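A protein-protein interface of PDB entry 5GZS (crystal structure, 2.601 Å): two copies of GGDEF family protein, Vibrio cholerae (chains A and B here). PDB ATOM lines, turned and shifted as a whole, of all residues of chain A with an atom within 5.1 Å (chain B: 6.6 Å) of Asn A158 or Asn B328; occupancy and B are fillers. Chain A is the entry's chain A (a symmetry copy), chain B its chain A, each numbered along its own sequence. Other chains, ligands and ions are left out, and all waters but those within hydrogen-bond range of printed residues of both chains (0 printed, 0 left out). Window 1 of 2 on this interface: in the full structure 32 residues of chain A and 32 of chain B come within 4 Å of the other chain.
The side-chain carboxylate (OD1) of Asp A159 is in hydrogen-bond range of the side-chain amide nitrogen (ND2) of Asn B328 (2.9 Å). The backbone carbonyl oxygen of Ile A163 is in hydrogen-bond range of the side-chain hydroxyl of Ser B330, 2.6 Å away.
N of Ser B327 is in hydrogen-bond range of OE2 of Glu B331 (3.0 Å). The side-chain amide oxygen (OD1) of Asn B328 sits close to the backbone NH (N) of Ser B330, 3.2 Å away. The backbone carbonyl oxygen (O) of Glu A77 sits at hydrogen-bond distance from the side-chain amide nitrogen (ND2) of Asn A158. The side-chain amide oxygen (OD1) of Asn A158 lies within hydrogen-bond range of the backbone NH (N) of Thr A79 (2.7 Å).
Among the printed residues, merely in contact across the chains: Asn A158 with Asn B328 (3.6 Å) and Asp A159 with Ser B327 (3.6 Å).
Of chain B, only Asn B328 (3.6 Å) comes within 4 Å of Asn A158. Of the printed residues of chain A, Asn B328 touches Asn A158 and Asp A159. Of the printed residues of chain A, Ser B327 touches Asp A159 (3.6 Å). Printed residues of chain B within 4 Å of Ile A163: Ser B330. Of the printed residues of chain A, Ser B330 touches Ile A163. Phe B408 touches none of the printed residues of chain A. Tyr A78 touches none of the printed residues of chain B. The nearest printed residue of chain A that does not touch Asn B328 is Ile A163 (5.4 Å). The nearest printed residue of chain B that does not touch Ile A163 is Asn B328 (5.4 Å).
Among the printed residues, 4 pairs touch across the chains. Among the printed residues, no Asp or Glu carboxylate lies within 4 Å of a Lys or Arg side-chain nitrogen of the other chain.
No position is printed for both chains.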
ATOM      1  N   GLU A  77     -34.547 -12.577  -4.155  1.00  0.00           N
ATOM      2  CA  GLU A  77     -35.023 -13.730  -4.888  1.00  0.00           C
ATOM      3  C   GLU A  77     -34.002 -14.065  -5.979  1.00  0.00           C
ATOM      4  O   GLU A  77     -33.766 -13.269  -6.891  1.00  0.00           O
ATOM      5  CB  GLU A  77     -36.402 -13.435  -5.470  1.00  0.00           C
ATOM      6  CG  GLU A  77     -37.050 -14.544  -6.259  1.00  0.00           C
ATOM      7  CD  GLU A  77     -38.314 -14.043  -6.952  1.00  0.00           C
ATOM      8  OE1 GLU A  77     -38.241 -12.936  -7.551  1.00  0.00           O
ATOM      9  OE2 GLU A  77     -39.365 -14.738  -6.904  1.00  0.00           O
ATOM     10  N   TYR A  78     -33.377 -15.230  -5.879  1.00  0.00           N
ATOM     11  CA  TYR A  78     -32.408 -15.632  -6.898  1.00  0.00           C
ATOM     12  C   TYR A  78     -33.136 -15.811  -8.239  1.00  0.00           C
ATOM     13  O   TYR A  78     -34.172 -16.487  -8.318  1.00  0.00           O
ATOM     14  CB  TYR A  78     -31.680 -16.908  -6.488  1.00  0.00           C
ATOM     15  CG  TYR A  78     -30.569 -16.701  -5.483  1.00  0.00           C
ATOM     16  CD1 TYR A  78     -30.839 -16.578  -4.127  1.00  0.00           C
ATOM     17  CD2 TYR A  78     -29.239 -16.653  -5.888  1.00  0.00           C
ATOM     18  CE1 TYR A  78     -29.818 -16.401  -3.217  1.00  0.00           C
ATOM     19  CE2 TYR A  78     -28.225 -16.477  -4.996  1.00  0.00           C
ATOM     20  CZ  TYR A  78     -28.507 -16.345  -3.667  1.00  0.00           C
ATOM     21  OH  TYR A  78     -27.469 -16.175  -2.766  1.00  0.00           O
ATOM     22  N   THR A  79     -32.591 -15.183  -9.278  1.00  0.00           N
ATOM     23  CA  THR A  79     -33.257 -15.098 -10.563  1.00  0.00           C
ATOM     24  C   THR A  79     -32.299 -15.464 -11.686  1.00  0.00           C
ATOM     25  O   THR A  79     -31.185 -14.942 -11.762  1.00  0.00           O
ATOM     26  CB  THR A  79     -33.835 -13.688 -10.800  1.00  0.00           C
ATOM     27  OG1 THR A  79     -34.876 -13.436  -9.841  1.00  0.00           O
ATOM     28  CG2 THR A  79     -34.419 -13.560 -12.223  1.00  0.00           C
ATOM     29  N   LEU A 156     -26.996 -16.521 -13.280  1.00  0.00           N
ATOM     30  CA  LEU A 156     -27.612 -15.737 -12.209  1.00  0.00           C
ATOM     31  C   LEU A 156     -27.759 -14.309 -12.665  1.00  0.00           C
ATOM     32  O   LEU A 156     -26.774 -13.669 -13.018  1.00  0.00           O
ATOM     33  CB  LEU A 156     -26.788 -15.783 -10.928  1.00  0.00           C
ATOM     34  CG  LEU A 156     -27.474 -15.134  -9.715  1.00  0.00           C
ATOM     35  CD1 LEU A 156     -28.831 -15.785  -9.517  1.00  0.00           C
ATOM     36  CD2 LEU A 156     -26.636 -15.234  -8.426  1.00  0.00           C
ATOM     37  N   LEU A 157     -28.987 -13.813 -12.676  1.00  0.00           N
ATOM     38  CA  LEU A 157     -29.229 -12.484 -13.191  1.00  0.00           C
ATOM     39  C   LEU A 157     -29.156 -11.409 -12.120  1.00  0.00           C
ATOM     40  O   LEU A 157     -29.223 -10.246 -12.452  1.00  0.00           O
ATOM     41  CB  LEU A 157     -30.597 -12.418 -13.893  1.00  0.00           C
ATOM     42  CG  LEU A 157     -30.762 -13.301 -15.147  1.00  0.00           C
ATOM     43  CD1 LEU A 157     -31.981 -12.895 -15.917  1.00  0.00           C
ATOM     44  CD2 LEU A 157     -29.523 -13.273 -16.066  1.00  0.00           C
ATOM     45  N   ASN A 158     -29.014 -11.775 -10.843  1.00  0.00           N
ATOM     46  CA  ASN A 158     -29.192 -10.792  -9.749  1.00  0.00           C
ATOM     47  C   ASN A 158     -28.083  -9.758  -9.685  1.00  0.00           C
ATOM     48  O   ASN A 158     -28.285  -8.647  -9.221  1.00  0.00           O
ATOM     49  CB  ASN A 158     -29.305 -11.487  -8.385  1.00  0.00           C
ATOM     50  CG  ASN A 158     -30.614 -12.233  -8.223  1.00  0.00           C
ATOM     51  OD1 ASN A 158     -30.723 -13.403  -8.610  1.00  0.00           O
ATOM     52  ND2 ASN A 158     -31.612 -11.570  -7.652  1.00  0.00           N
ATOM     53  N   ASP A 159     -26.904 -10.127 -10.147  1.00  0.00           N
ATOM     54  CA  ASP A 159     -25.813  -9.178 -10.183  1.00  0.00           C
ATOM     55  C   ASP A 159     -25.615  -8.631 -11.599  1.00  0.00           C
ATOM     56  O   ASP A 159     -24.586  -8.055 -11.909  1.00  0.00           O
ATOM     57  CB  ASP A 159     -24.564  -9.854  -9.637  1.00  0.00           C
ATOM     58  CG  ASP A 159     -24.806 -10.476  -8.246  1.00  0.00           C
ATOM     59  OD1 ASP A 159     -25.360  -9.784  -7.360  1.00  0.00           O
ATOM     60  OD2 ASP A 159     -24.451 -11.656  -8.035  1.00  0.00           O
ATOM     61  N   GLN A 160     -26.642  -8.803 -12.435  1.00  0.00           N
ATOM     62  CA  GLN A 160     -26.628  -8.407 -13.840  1.00  0.00           C
ATOM     63  C   GLN A 160     -27.676  -7.331 -14.087  1.00  0.00           C
ATOM     64  O   GLN A 160     -27.563  -6.504 -14.985  1.00  0.00           O
ATOM     65  CB  GLN A 160     -26.938  -9.608 -14.749  1.00  0.00           C
ATOM     66  CG  GLN A 160     -25.921 -10.703 -14.713  1.00  0.00           C
ATOM     67  CD  GLN A 160     -24.753 -10.420 -15.615  1.00  0.00           C
ATOM     68  OE1 GLN A 160     -24.456  -9.265 -15.918  1.00  0.00           O
ATOM     69  NE2 GLN A 160     -24.071 -11.475 -16.049  1.00  0.00           N
ATOM     70  N   LEU A 161     -28.729  -7.392 -13.292  1.00  0.00           N
ATOM     71  CA  LEU A 161     -29.879  -6.534 -13.469  1.00  0.00           C
ATOM     72  C   LEU A 161     -30.365  -6.130 -12.105  1.00  0.00           C
ATOM     73  O   LEU A 161     -30.182  -6.861 -11.146  1.00  0.00           O
ATOM     74  CB  LEU A 161     -30.992  -7.242 -14.229  1.00  0.00           C
ATOM     75  CG  LEU A 161     -30.857  -7.472 -15.726  1.00  0.00           C
ATOM     76  CD1 LEU A 161     -32.073  -8.246 -16.231  1.00  0.00           C
ATOM     77  CD2 LEU A 161     -30.754  -6.144 -16.443  1.00  0.00           C
ATOM     78  N   ILE A 163     -32.594  -6.590  -9.715  1.00  0.00           N
ATOM     79  CA  ILE A 163     -33.709  -7.451  -9.313  1.00  0.00           C
ATOM     80  C   ILE A 163     -34.290  -6.988  -8.003  1.00  0.00           C
ATOM     81  O   ILE A 163     -33.650  -7.077  -6.976  1.00  0.00           O
ATOM     82  CB  ILE A 163     -33.299  -8.918  -9.167  1.00  0.00           C
ATOM     83  CG1 ILE A 163     -32.720  -9.439 -10.487  1.00  0.00           C
ATOM     84  CG2 ILE A 163     -34.510  -9.754  -8.728  1.00  0.00           C
ATOM     85  CD1 ILE A 163     -33.751  -9.469 -11.632  1.00  0.00           C
ATOM     86  N   TYR B 326     -22.768  -7.526   1.680  1.00  0.00           N
ATOM     87  CA  TYR B 326     -23.722  -7.293   0.600  1.00  0.00           C
ATOM     88  C   TYR B 326     -23.029  -6.860  -0.675  1.00  0.00           C
ATOM     89  O   TYR B 326     -22.132  -6.022  -0.646  1.00  0.00           O
ATOM     90  CB  TYR B 326     -24.741  -6.226   0.991  1.00  0.00           C
ATOM     91  CG  TYR B 326     -25.310  -6.357   2.373  1.00  0.00           C
ATOM     92  CD1 TYR B 326     -26.204  -7.373   2.679  1.00  0.00           C
ATOM     93  CD2 TYR B 326     -24.986  -5.437   3.370  1.00  0.00           C
ATOM     94  CE1 TYR B 326     -26.750  -7.486   3.945  1.00  0.00           C
ATOM     95  CE2 TYR B 326     -25.531  -5.540   4.637  1.00  0.00           C
ATOM     96  CZ  TYR B 326     -26.409  -6.571   4.916  1.00  0.00           C
ATOM     97  OH  TYR B 326     -26.947  -6.687   6.167  1.00  0.00           O
ATOM     98  N   SER B 327     -23.475  -7.397  -1.801  1.00  0.00           N
ATOM     99  CA  SER B 327     -22.806  -7.119  -3.055  1.00  0.00           C
ATOM    100  C   SER B 327     -23.657  -6.230  -3.952  1.00  0.00           C
ATOM    101  O   SER B 327     -23.117  -5.561  -4.843  1.00  0.00           O
ATOM    102  CB  SER B 327     -22.447  -8.418  -3.758  1.00  0.00           C
ATOM    103  OG  SER B 327     -23.599  -9.037  -4.289  1.00  0.00           O
ATOM    104  N   ASN B 328     -24.973  -6.200  -3.714  1.00  0.00           N
ATOM    105  CA  ASN B 328     -25.810  -5.132  -4.290  1.00  0.00           C
ATOM    106  C   ASN B 328     -27.027  -4.706  -3.438  1.00  0.00           C
ATOM    107  O   ASN B 328     -27.481  -5.430  -2.571  1.00  0.00           O
ATOM    108  CB  ASN B 328     -26.262  -5.526  -5.698  1.00  0.00           C
ATOM    109  CG  ASN B 328     -27.330  -6.564  -5.690  1.00  0.00           C
ATOM    110  OD1 ASN B 328     -28.499  -6.250  -5.467  1.00  0.00           O
ATOM    111  ND2 ASN B 328     -26.950  -7.824  -5.938  1.00  0.00           N
ATOM    112  N   VAL B 329     -27.567  -3.525  -3.726  1.00  0.00           N
ATOM    113  CA  VAL B 329     -28.440  -2.822  -2.791  1.00  0.00           C
ATOM    114  C   VAL B 329     -29.772  -3.529  -2.498  1.00  0.00           C
ATOM    115  O   VAL B 329     -30.393  -3.285  -1.460  1.00  0.00           O
ATOM    116  CB  VAL B 329     -28.702  -1.356  -3.284  1.00  0.00           C
ATOM    117  CG1 VAL B 329     -29.434  -1.312  -4.623  1.00  0.00           C
ATOM    118  CG2 VAL B 329     -29.442  -0.548  -2.226  1.00  0.00           C
ATOM    119  N   SER B 330     -30.191  -4.437  -3.373  1.00  0.00           N
ATOM    120  CA  SER B 330     -31.369  -5.275  -3.102  1.00  0.00           C
ATOM    121  C   SER B 330     -31.223  -6.145  -1.854  1.00  0.00           C
ATOM    122  O   SER B 330     -32.212  -6.598  -1.270  1.00  0.00           O
ATOM    123  CB  SER B 330     -31.670  -6.182  -4.289  1.00  0.00           C
ATOM    124  OG  SER B 330     -32.511  -5.526  -5.211  1.00  0.00           O
ATOM    125  N   GLU B 331     -29.984  -6.385  -1.449  1.00  0.00           N
ATOM    126  CA  GLU B 331     -29.735  -7.194  -0.270  1.00  0.00           C
ATOM    127  C   GLU B 331     -29.729  -6.341   1.012  1.00  0.00           C
ATOM    128  O   GLU B 331     -29.301  -6.827   2.064  1.00  0.00           O
ATOM    129  CB  GLU B 331     -28.413  -7.952  -0.439  1.00  0.00           C
ATOM    130  CG  GLU B 331     -28.438  -8.951  -1.597  1.00  0.00           C
ATOM    131  CD  GLU B 331     -27.056  -9.372  -2.043  1.00  0.00           C
ATOM    132  OE1 GLU B 331     -26.935 -10.190  -2.985  1.00  0.00           O
ATOM    133  OE2 GLU B 331     -26.077  -8.884  -1.449  1.00  0.00           O
ATOM    134  N   LEU B 332     -30.208  -5.088   0.928  1.00  0.00           N
ATOM    135  CA  LEU B 332     -30.302  -4.209   2.111  1.00  0.00           C
ATOM    136  C   LEU B 332     -31.703  -4.164   2.715  1.00  0.00           C
ATOM    137  O   LEU B 332     -32.081  -3.209   3.404  1.00  0.00           O
ATOM    138  CB  LEU B 332     -29.855  -2.786   1.780  1.00  0.00           C
ATOM    139  CG  LEU B 332     -28.464  -2.549   2.368  1.00  0.00           C
ATOM    140  CD1 LEU B 332     -27.578  -3.742   2.077  1.00  0.00           C
ATOM    141  CD2 LEU B 332     -27.837  -1.332   1.830  1.00  0.00           C
ATOM    142  N   MET B 404     -18.346  -2.721  -2.315  1.00  0.00           N
ATOM    143  CA  MET B 404     -18.880  -3.984  -2.758  1.00  0.00           C
ATOM    144  C   MET B 404     -20.102  -3.685  -3.539  1.00  0.00           C
ATOM    145  O   MET B 404     -20.252  -4.126  -4.659  1.00  0.00           O
ATOM    146  CB  MET B 404     -19.211  -4.881  -1.566  1.00  0.00           C
ATOM    147  CG  MET B 404     -19.642  -6.284  -1.959  1.00  0.00           C
ATOM    148  SD  MET B 404     -18.235  -7.587  -1.930  1.00  0.00           S
ATOM    149  CE  MET B 404     -17.446  -7.184  -3.667  1.00  0.00           C
ATOM    150  N   ILE B 405     -20.999  -2.932  -2.952  1.00  0.00           N
ATOM    151  CA  ILE B 405     -22.195  -2.646  -3.665  1.00  0.00           C
ATOM    152  C   ILE B 405     -21.753  -1.760  -4.792  1.00  0.00           C
ATOM    153  O   ILE B 405     -22.187  -1.910  -5.907  1.00  0.00           O
ATOM    154  CB  ILE B 405     -23.221  -1.989  -2.747  1.00  0.00           C
ATOM    155  CG1 ILE B 405     -23.926  -3.043  -1.910  1.00  0.00           C
ATOM    156  CG2 ILE B 405     -24.261  -1.223  -3.541  1.00  0.00           C
ATOM    157  CD1 ILE B 405     -24.117  -2.663  -0.477  1.00  0.00           C
ATOM    158  N   GLY B 406     -20.864  -0.839  -4.491  1.00  0.00           N
ATOM    159  CA  GLY B 406     -20.479   0.139  -5.471  1.00  0.00           C
ATOM    160  C   GLY B 406     -21.621   0.952  -6.035  1.00  0.00           C
ATOM    161  O   GLY B 406     -22.672   1.093  -5.476  1.00  0.00           O
ATOM    162  N   PHE B 408     -24.567   1.546  -7.453  1.00  0.00           N
ATOM    163  CA  PHE B 408     -25.747   0.736  -7.640  1.00  0.00           C
ATOM    164  C   PHE B 408     -26.708   1.376  -8.619  1.00  0.00           C
ATOM    165  O   PHE B 408     -27.732   0.780  -8.938  1.00  0.00           O
ATOM    166  CB  PHE B 408     -26.448   0.500  -6.305  1.00  0.00           C
ATOM    167  CG  PHE B 408     -27.010   1.746  -5.685  1.00  0.00           C
ATOM    168  CD1 PHE B 408     -26.201   2.590  -4.929  1.00  0.00           C
ATOM    169  CD2 PHE B 408     -28.340   2.068  -5.852  1.00  0.00           C
ATOM    170  CE1 PHE B 408     -26.708   3.729  -4.356  1.00  0.00           C
ATOM    171  CE2 PHE B 408     -28.868   3.208  -5.282  1.00  0.00           C
ATOM    172  CZ  PHE B 408     -28.048   4.044  -4.525  1.00  0.00           C
